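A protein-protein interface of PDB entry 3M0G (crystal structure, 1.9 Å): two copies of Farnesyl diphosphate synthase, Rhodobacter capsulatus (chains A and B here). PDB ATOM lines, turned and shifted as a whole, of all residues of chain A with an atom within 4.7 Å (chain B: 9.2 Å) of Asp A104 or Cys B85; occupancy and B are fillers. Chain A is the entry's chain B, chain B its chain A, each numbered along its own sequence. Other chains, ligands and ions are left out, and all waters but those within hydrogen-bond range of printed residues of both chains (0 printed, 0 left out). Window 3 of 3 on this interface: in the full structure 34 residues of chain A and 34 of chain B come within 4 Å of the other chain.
SG of Cys B85 sits at hydrogen-bond distance from N of Ala A105 (3.8 Å).
The backbone carbonyl oxygen (O) of Val B108 sits at hydrogen-bond distance from a ring nitrogen (NE2) of His B80 (2.8 Å). The backbone NH (N) of Asn B88 lies within hydrogen-bond range of the backbone carbonyl oxygen (O) of Met B83, at 3.0 Å.
Val B108 touches Met A83 (CG1 to CE, 3.4 Å). Asp A104 touches Cys B85. His B80 touches Val A108 (ND1 to CG1, 3.6 Å). Val A108 touches Met B83.
Printed residues of chain B within 4 Å of Asp A104: Cys B85 (3.8 Å). Cys B85 touches just these residues of chain A: Asp A104 (3.8 Å) and Ala A105 (3.5 Å). No residue of chain B comes within 4 Å of Asp A103. Of chain B, only Cys B85 comes within 4 Å of Ala A105. No residue of chain B comes within 4 Å of Ala A107. Of the printed residues of chain A, His B80 touches Val A108 (3.6 Å). Of the printed residues of chain B, Met A83 touches Val B108 (3.4 Å). Of the printed residues of chain A, Val B108 touches Met A83. Printed residues of chain A within 4 Å of Met B83: Val A108. Printed residues of chain B within 4 Å of Val A108: His B80 and Met B83. Asp B104 touches none of the printed residues of chain A. The nearest printed residue of chain B that does not touch Asp A104 is Met B83 (6.3 Å). The nearest residue of chain A that does not touch Cys B85 is Val A108 (4.1 Å).
Hydrophobic or aromatic side chains of chain A within 4 Å of the printed part of chain B: Met A83, Ala A105 and Val A108. Of the 17 printed residues of chain B, 4 touch a printed residue of chain A. Printed residues of chain B that touch a printed residue of chain A: His B80, Met B83, Cys B85 and Val B108. Hydrophobic or aromatic side chains of chain B that line the printed part of chain A: His B80, Met B83 and Val B108. Among the printed residues, 5 pairs touch across the chains.
Met A83 touches Val B108, and with the chains exchanged Val A108 touches Met B83. Positions printed for both chains: 83, 84, 99, 104 and 108. Of the 5 pairs that touch across the chains among the printed residues, 2 have their exchanged pair printed and touching as well.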
ATOM      1  N   MET A  83      12.975  17.963 -29.598  1.00  0.00           N
ATOM      2  CA  MET A  83      13.417  19.234 -29.001  1.00  0.00           C
ATOM      3  C   MET A  83      13.054  20.447 -29.867  1.00  0.00           C
ATOM      4  O   MET A  83      12.976  20.324 -31.096  1.00  0.00           O
ATOM      5  CB  MET A  83      14.919  19.227 -28.673  1.00  0.00           C
ATOM      6  CG  MET A  83      15.325  18.293 -27.563  1.00  0.00           C
ATOM      7  SD  MET A  83      17.258  18.322 -27.251  1.00  0.00           S
ATOM      8  CE  MET A  83      17.859  18.245 -29.080  1.00  0.00           C
ATOM      9  N   PRO A  84      12.851  21.620 -29.224  1.00  0.00           N
ATOM     10  CA  PRO A  84      12.383  22.858 -29.873  1.00  0.00           C
ATOM     11  C   PRO A  84      13.188  23.245 -31.116  1.00  0.00           C
ATOM     12  O   PRO A  84      12.600  23.616 -32.129  1.00  0.00           O
ATOM     13  CB  PRO A  84      12.533  23.910 -28.768  1.00  0.00           C
ATOM     14  CG  PRO A  84      12.369  23.115 -27.494  1.00  0.00           C
ATOM     15  CD  PRO A  84      13.088  21.829 -27.779  1.00  0.00           C
ATOM     16  N   HIS A  99      11.669  16.701 -23.094  1.00  0.00           N
ATOM     17  CA  HIS A  99      12.088  18.086 -22.924  1.00  0.00           C
ATOM     18  C   HIS A  99      10.965  18.935 -22.277  1.00  0.00           C
ATOM     19  O   HIS A  99      11.254  19.899 -21.579  1.00  0.00           O
ATOM     20  CB  HIS A  99      12.602  18.675 -24.235  1.00  0.00           C
ATOM     21  CG  HIS A  99      11.536  19.269 -25.099  1.00  0.00           C
ATOM     22  ND1 HIS A  99      10.855  18.544 -26.052  1.00  0.00           N
ATOM     23  CD2 HIS A  99      11.047  20.528 -25.162  1.00  0.00           C
ATOM     24  CE1 HIS A  99       9.982  19.329 -26.656  1.00  0.00           C
ATOM     25  NE2 HIS A  99      10.080  20.537 -26.134  1.00  0.00           N
ATOM     26  N   ASP A 103      13.400  19.257 -18.840  1.00  0.00           N
ATOM     27  CA  ASP A 103      13.751  20.475 -19.562  1.00  0.00           C
ATOM     28  C   ASP A 103      14.627  20.108 -20.759  1.00  0.00           C
ATOM     29  O   ASP A 103      14.877  18.919 -20.988  1.00  0.00           O
ATOM     30  CB  ASP A 103      14.404  21.528 -18.639  1.00  0.00           C
ATOM     31  CG  ASP A 103      15.583  20.984 -17.830  1.00  0.00           C
ATOM     32  OD1 ASP A 103      16.197  19.975 -18.231  1.00  0.00           O
ATOM     33  OD2 ASP A 103      15.925  21.609 -16.797  1.00  0.00           O
ATOM     34  N   ASP A 104      15.065  21.107 -21.526  1.00  0.00           N
ATOM     35  CA  ASP A 104      15.909  20.870 -22.703  1.00  0.00           C
ATOM     36  C   ASP A 104      17.251  20.206 -22.349  1.00  0.00           C
ATOM     37  O   ASP A 104      17.699  19.291 -23.046  1.00  0.00           O
ATOM     38  CB  ASP A 104      16.141  22.171 -23.485  1.00  0.00           C
ATOM     39  CG  ASP A 104      14.939  22.581 -24.318  1.00  0.00           C
ATOM     40  OD1 ASP A 104      13.893  21.930 -24.239  1.00  0.00           O
ATOM     41  OD2 ASP A 104      15.044  23.588 -25.049  1.00  0.00           O
ATOM     42  N   ALA A 105      17.882  20.670 -21.271  1.00  0.00           N
ATOM     43  CA  ALA A 105      19.150  20.094 -20.795  1.00  0.00           C
ATOM     44  C   ALA A 105      19.017  18.592 -20.530  1.00  0.00           C
ATOM     45  O   ALA A 105      19.861  17.793 -20.960  1.00  0.00           O
ATOM     46  CB  ALA A 105      19.620  20.807 -19.534  1.00  0.00           C
ATOM     47  N   THR A 106      17.956  18.223 -19.813  1.00  0.00           N
ATOM     48  CA  THR A 106      17.659  16.815 -19.521  1.00  0.00           C
ATOM     49  C   THR A 106      17.388  15.965 -20.770  1.00  0.00           C
ATOM     50  O   THR A 106      17.822  14.804 -20.827  1.00  0.00           O
ATOM     51  CB  THR A 106      16.516  16.676 -18.501  1.00  0.00           C
ATOM     52  OG1 THR A 106      16.800  17.509 -17.369  1.00  0.00           O
ATOM     53  CG2 THR A 106      16.368  15.229 -18.043  1.00  0.00           C
ATOM     54  N   ALA A 107      16.684  16.521 -21.765  1.00  0.00           N
ATOM     55  CA  ALA A 107      16.513  15.818 -23.041  1.00  0.00           C
ATOM     56  C   ALA A 107      17.830  15.588 -23.819  1.00  0.00           C
ATOM     57  O   ALA A 107      18.050  14.521 -24.369  1.00  0.00           O
ATOM     58  CB  ALA A 107      15.459  16.533 -23.933  1.00  0.00           C
ATOM     59  N   VAL A 108      18.703  16.584 -23.875  1.00  0.00           N
ATOM     60  CA  VAL A 108      20.031  16.376 -24.464  1.00  0.00           C
ATOM     61  C   VAL A 108      20.715  15.205 -23.762  1.00  0.00           C
ATOM     62  O   VAL A 108      21.167  14.242 -24.397  1.00  0.00           O
ATOM     63  CB  VAL A 108      20.904  17.645 -24.328  1.00  0.00           C
ATOM     64  CG1 VAL A 108      22.374  17.395 -24.794  1.00  0.00           C
ATOM     65  CG2 VAL A 108      20.262  18.799 -25.041  1.00  0.00           C
ATOM     66  N   VAL B  79      30.534  19.926 -27.531  1.00  0.00           N
ATOM     67  CA  VAL B  79      29.524  20.468 -28.431  1.00  0.00           C
ATOM     68  C   VAL B  79      28.178  20.566 -27.707  1.00  0.00           C
ATOM     69  O   VAL B  79      27.518  21.600 -27.789  1.00  0.00           O
ATOM     70  CB  VAL B  79      29.413  19.595 -29.699  1.00  0.00           C
ATOM     71  CG1 VAL B  79      28.338  20.106 -30.631  1.00  0.00           C
ATOM     72  CG2 VAL B  79      30.724  19.569 -30.425  1.00  0.00           C
ATOM     73  N   HIS B  80      27.769  19.491 -27.015  1.00  0.00           N
ATOM     74  CA  HIS B  80      26.518  19.517 -26.255  1.00  0.00           C
ATOM     75  C   HIS B  80      26.567  20.441 -25.030  1.00  0.00           C
ATOM     76  O   HIS B  80      25.651  21.231 -24.810  1.00  0.00           O
ATOM     77  CB  HIS B  80      26.047  18.105 -25.869  1.00  0.00           C
ATOM     78  CG  HIS B  80      25.439  17.354 -27.015  1.00  0.00           C
ATOM     79  ND1 HIS B  80      24.919  16.082 -26.893  1.00  0.00           N
ATOM     80  CD2 HIS B  80      25.294  17.695 -28.318  1.00  0.00           C
ATOM     81  CE1 HIS B  80      24.461  15.680 -28.068  1.00  0.00           C
ATOM     82  NE2 HIS B  80      24.686  16.639 -28.953  1.00  0.00           N
ATOM     83  N   ASP B  81      27.626  20.329 -24.248  1.00  0.00           N
ATOM     84  CA  ASP B  81      27.747  21.093 -23.010  1.00  0.00           C
ATOM     85  C   ASP B  81      27.835  22.595 -23.240  1.00  0.00           C
ATOM     86  O   ASP B  81      27.429  23.383 -22.371  1.00  0.00           O
ATOM     87  CB  ASP B  81      28.939  20.617 -22.188  1.00  0.00           C
ATOM     88  CG  ASP B  81      28.781  19.198 -21.697  1.00  0.00           C
ATOM     89  OD1 ASP B  81      27.681  18.616 -21.858  1.00  0.00           O
ATOM     90  OD2 ASP B  81      29.762  18.660 -21.151  1.00  0.00           O
ATOM     91  N   ASP B  82      28.364  22.978 -24.404  1.00  0.00           N
ATOM     92  CA  ASP B  82      28.479  24.381 -24.817  1.00  0.00           C
ATOM     93  C   ASP B  82      27.100  25.015 -25.096  1.00  0.00           C
ATOM     94  O   ASP B  82      26.962  26.239 -25.072  1.00  0.00           O
ATOM     95  CB  ASP B  82      29.366  24.512 -26.070  1.00  0.00           C
ATOM     96  CG  ASP B  82      30.879  24.472 -25.769  1.00  0.00           C
ATOM     97  OD1 ASP B  82      31.296  24.516 -24.588  1.00  0.00           O
ATOM     98  OD2 ASP B  82      31.670  24.408 -26.744  1.00  0.00           O
ATOM     99  N   MET B  83      26.085  24.185 -25.325  1.00  0.00           N
ATOM    100  CA  MET B  83      24.753  24.665 -25.752  1.00  0.00           C
ATOM    101  C   MET B  83      24.021  25.582 -24.752  1.00  0.00           C
ATOM    102  O   MET B  83      24.298  25.555 -23.539  1.00  0.00           O
ATOM    103  CB  MET B  83      23.847  23.497 -26.183  1.00  0.00           C
ATOM    104  CG  MET B  83      24.304  22.781 -27.458  1.00  0.00           C
ATOM    105  SD  MET B  83      23.135  21.282 -27.953  1.00  0.00           S
ATOM    106  CE  MET B  83      23.018  20.343 -26.269  1.00  0.00           C
ATOM    107  N   PRO B  84      23.106  26.426 -25.271  1.00  0.00           N
ATOM    108  CA  PRO B  84      22.364  27.390 -24.447  1.00  0.00           C
ATOM    109  C   PRO B  84      21.644  26.819 -23.213  1.00  0.00           C
ATOM    110  O   PRO B  84      21.625  27.479 -22.165  1.00  0.00           O
ATOM    111  CB  PRO B  84      21.391  28.012 -25.451  1.00  0.00           C
ATOM    112  CG  PRO B  84      22.200  28.035 -26.721  1.00  0.00           C
ATOM    113  CD  PRO B  84      22.871  26.671 -26.709  1.00  0.00           C
ATOM    114  N   CYS B  85      21.097  25.609 -23.313  1.00  0.00           N
ATOM    115  CA  CYS B  85      20.428  24.979 -22.165  1.00  0.00           C
ATOM    116  C   CYS B  85      21.403  24.401 -21.136  1.00  0.00           C
ATOM    117  O   CYS B  85      20.994  23.977 -20.050  1.00  0.00           O
ATOM    118  CB  CYS B  85      19.441  23.907 -22.630  1.00  0.00           C
ATOM    119  SG  CYS B  85      20.172  22.577 -23.583  1.00  0.00           S
ATOM    120  N   MET B  86      22.692  24.398 -21.478  1.00  0.00           N
ATOM    121  CA  MET B  86      23.722  23.826 -20.620  1.00  0.00           C
ATOM    122  C   MET B  86      24.689  24.922 -20.156  1.00  0.00           C
ATOM    123  O   MET B  86      24.277  25.824 -19.436  1.00  0.00           O
ATOM    124  CB  MET B  86      24.441  22.688 -21.342  1.00  0.00           C
ATOM    125  CG  MET B  86      23.517  21.557 -21.851  1.00  0.00           C
ATOM    126  SD  MET B  86      23.567  19.898 -20.787  1.00  0.00           S
ATOM    127  CE  MET B  86      25.450  19.814 -20.446  1.00  0.00           C
ATOM    128  N   ASP B  87      25.954  24.861 -20.563  1.00  0.00           N
ATOM    129  CA  ASP B  87      26.953  25.848 -20.103  1.00  0.00           C
ATOM    130  C   ASP B  87      26.845  27.201 -20.832  1.00  0.00           C
ATOM    131  O   ASP B  87      27.334  28.224 -20.334  1.00  0.00           O
ATOM    132  CB  ASP B  87      28.384  25.302 -20.200  1.00  0.00           C
ATOM    133  CG  ASP B  87      28.611  24.040 -19.362  1.00  0.00           C
ATOM    134  OD1 ASP B  87      27.783  23.695 -18.484  1.00  0.00           O
ATOM    135  OD2 ASP B  87      29.649  23.385 -19.592  1.00  0.00           O
ATOM    136  N   ASN B  88      26.202  27.206 -22.000  1.00  0.00           N
ATOM    137  CA  ASN B  88      25.926  28.447 -22.745  1.00  0.00           C
ATOM    138  C   ASN B  88      27.198  29.270 -22.994  1.00  0.00           C
ATOM    139  O   ASN B  88      27.304  30.425 -22.562  1.00  0.00           O
ATOM    140  CB  ASN B  88      24.840  29.271 -22.021  1.00  0.00           C
ATOM    141  CG  ASN B  88      24.342  30.467 -22.836  1.00  0.00           C
ATOM    142  OD1 ASN B  88      24.030  31.520 -22.271  1.00  0.00           O
ATOM    143  ND2 ASN B  88      24.251  30.304 -24.156  1.00  0.00           N
ATOM    144  N   ASP B  89      28.166  28.653 -23.668  1.00  0.00           N
ATOM    145  CA  ASP B  89      29.405  29.324 -24.062  1.00  0.00           C
ATOM    146  C   ASP B  89      29.354  29.733 -25.536  1.00  0.00           C
ATOM    147  O   ASP B  89      28.951  28.950 -26.393  1.00  0.00           O
ATOM    148  CB  ASP B  89      30.631  28.437 -23.792  1.00  0.00           C
ATOM    149  CG  ASP B  89      30.754  28.027 -22.330  1.00  0.00           C
ATOM    150  OD1 ASP B  89      30.962  28.904 -21.462  1.00  0.00           O
ATOM    151  OD2 ASP B  89      30.661  26.818 -22.051  1.00  0.00           O
ATOM    152  N   HIS B  99      27.242  25.662 -31.984  1.00  0.00           N
ATOM    153  CA  HIS B  99      25.854  26.144 -32.075  1.00  0.00           C
ATOM    154  C   HIS B  99      25.807  27.620 -32.473  1.00  0.00           C
ATOM    155  O   HIS B  99      24.792  28.102 -32.992  1.00  0.00           O
ATOM    156  CB  HIS B  99      25.089  25.928 -30.767  1.00  0.00           C
ATOM    157  CG  HIS B  99      25.561  26.789 -29.636  1.00  0.00           C
ATOM    158  ND1 HIS B  99      26.641  26.456 -28.848  1.00  0.00           N
ATOM    159  CD2 HIS B  99      25.094  27.966 -29.158  1.00  0.00           C
ATOM    160  CE1 HIS B  99      26.813  27.385 -27.923  1.00  0.00           C
ATOM    161  NE2 HIS B  99      25.892  28.320 -28.095  1.00  0.00           N
ATOM    162  N   ASP B 104      21.774  25.574 -33.165  1.00  0.00           N
ATOM    163  CA  ASP B 104      21.560  24.677 -32.027  1.00  0.00           C
ATOM    164  C   ASP B 104      21.282  23.273 -32.504  1.00  0.00           C
ATOM    165  O   ASP B 104      21.757  22.309 -31.900  1.00  0.00           O
ATOM    166  CB  ASP B 104      20.409  25.140 -31.125  1.00  0.00           C
ATOM    167  CG  ASP B 104      20.815  26.251 -30.177  1.00  0.00           C
ATOM    168  OD1 ASP B 104      21.902  26.830 -30.373  1.00  0.00           O
ATOM    169  OD2 ASP B 104      20.050  26.537 -29.228  1.00  0.00           O
ATOM    170  N   VAL B 108      23.422  19.725 -31.720  1.00  0.00           N
ATOM    171  CA  VAL B 108      22.794  18.483 -31.241  1.00  0.00           C
ATOM    172  C   VAL B 108      23.263  17.333 -32.101  1.00  0.00           C
ATOM    173  O   VAL B 108      23.819  16.354 -31.600  1.00  0.00           O
ATOM    174  CB  VAL B 108      21.235  18.556 -31.224  1.00  0.00           C
ATOM    175  CG1 VAL B 108      20.636  17.234 -30.717  1.00  0.00           C
ATOM    176  CG2 VAL B 108      20.753  19.727 -30.403  1.00  0.00           C
ATOM    177  N   GLN B 153      27.678  14.971 -15.601  1.00  0.00           N
ATOM    178  CA  GLN B 153      27.171  16.224 -16.160  1.00  0.00           C
ATOM    179  C   GLN B 153      25.760  16.570 -15.632  1.00  0.00           C
ATOM    180  O   GLN B 153      25.439  17.740 -15.412  1.00  0.00           O
ATOM    181  CB  GLN B 153      27.183  16.171 -17.686  1.00  0.00           C
ATOM    182  CG  GLN B 153      26.612  17.400 -18.366  1.00  0.00           C
ATOM    183  CD  GLN B 153      27.497  18.625 -18.245  1.00  0.00           C
ATOM    184  OE1 GLN B 153      27.103  19.634 -17.657  1.00  0.00           O
ATOM    185  NE2 GLN B 153      28.693  18.548 -18.808  1.00  0.00           N
ATOM    186  N   ILE B 157      24.616  19.990 -13.420  1.00  0.00           N
ATOM    187  CA  ILE B 157      23.494  20.890 -13.717  1.00  0.00           C
ATOM    188  C   ILE B 157      22.568  21.082 -12.503  1.00  0.00           C
ATOM    189  O   ILE B 157      22.071  22.188 -12.268  1.00  0.00           O
ATOM    190  CB  ILE B 157      22.665  20.426 -14.961  1.00  0.00           C
ATOM    191  CG1 ILE B 157      23.531  20.362 -16.236  1.00  0.00           C
ATOM    192  CG2 ILE B 157      21.419  21.307 -15.162  1.00  0.00           C
ATOM    193  CD1 ILE B 157      24.250  21.675 -16.623  1.00  0.00           C
ATOM    194  N   GLU B 160      24.148  23.652  -9.394  1.00  0.00           N
ATOM    195  CA  GLU B 160      24.054  25.117  -9.479  1.00  0.00           C
ATOM    196  C   GLU B 160      22.648  25.691  -9.260  1.00  0.00           C
ATOM    197  O   GLU B 160      22.438  26.900  -9.383  1.00  0.00           O
ATOM    198  CB  GLU B 160      24.649  25.622 -10.798  1.00  0.00           C
ATOM    199  CG  GLU B 160      24.087  24.962 -12.056  1.00  0.00           C
ATOM    200  CD  GLU B 160      25.089  24.948 -13.199  1.00  0.00           C
ATOM    201  OE1 GLU B 160      24.656  24.797 -14.359  1.00  0.00           O
ATOM    202  OE2 GLU B 160      26.310  25.091 -12.935  1.00  0.00           O
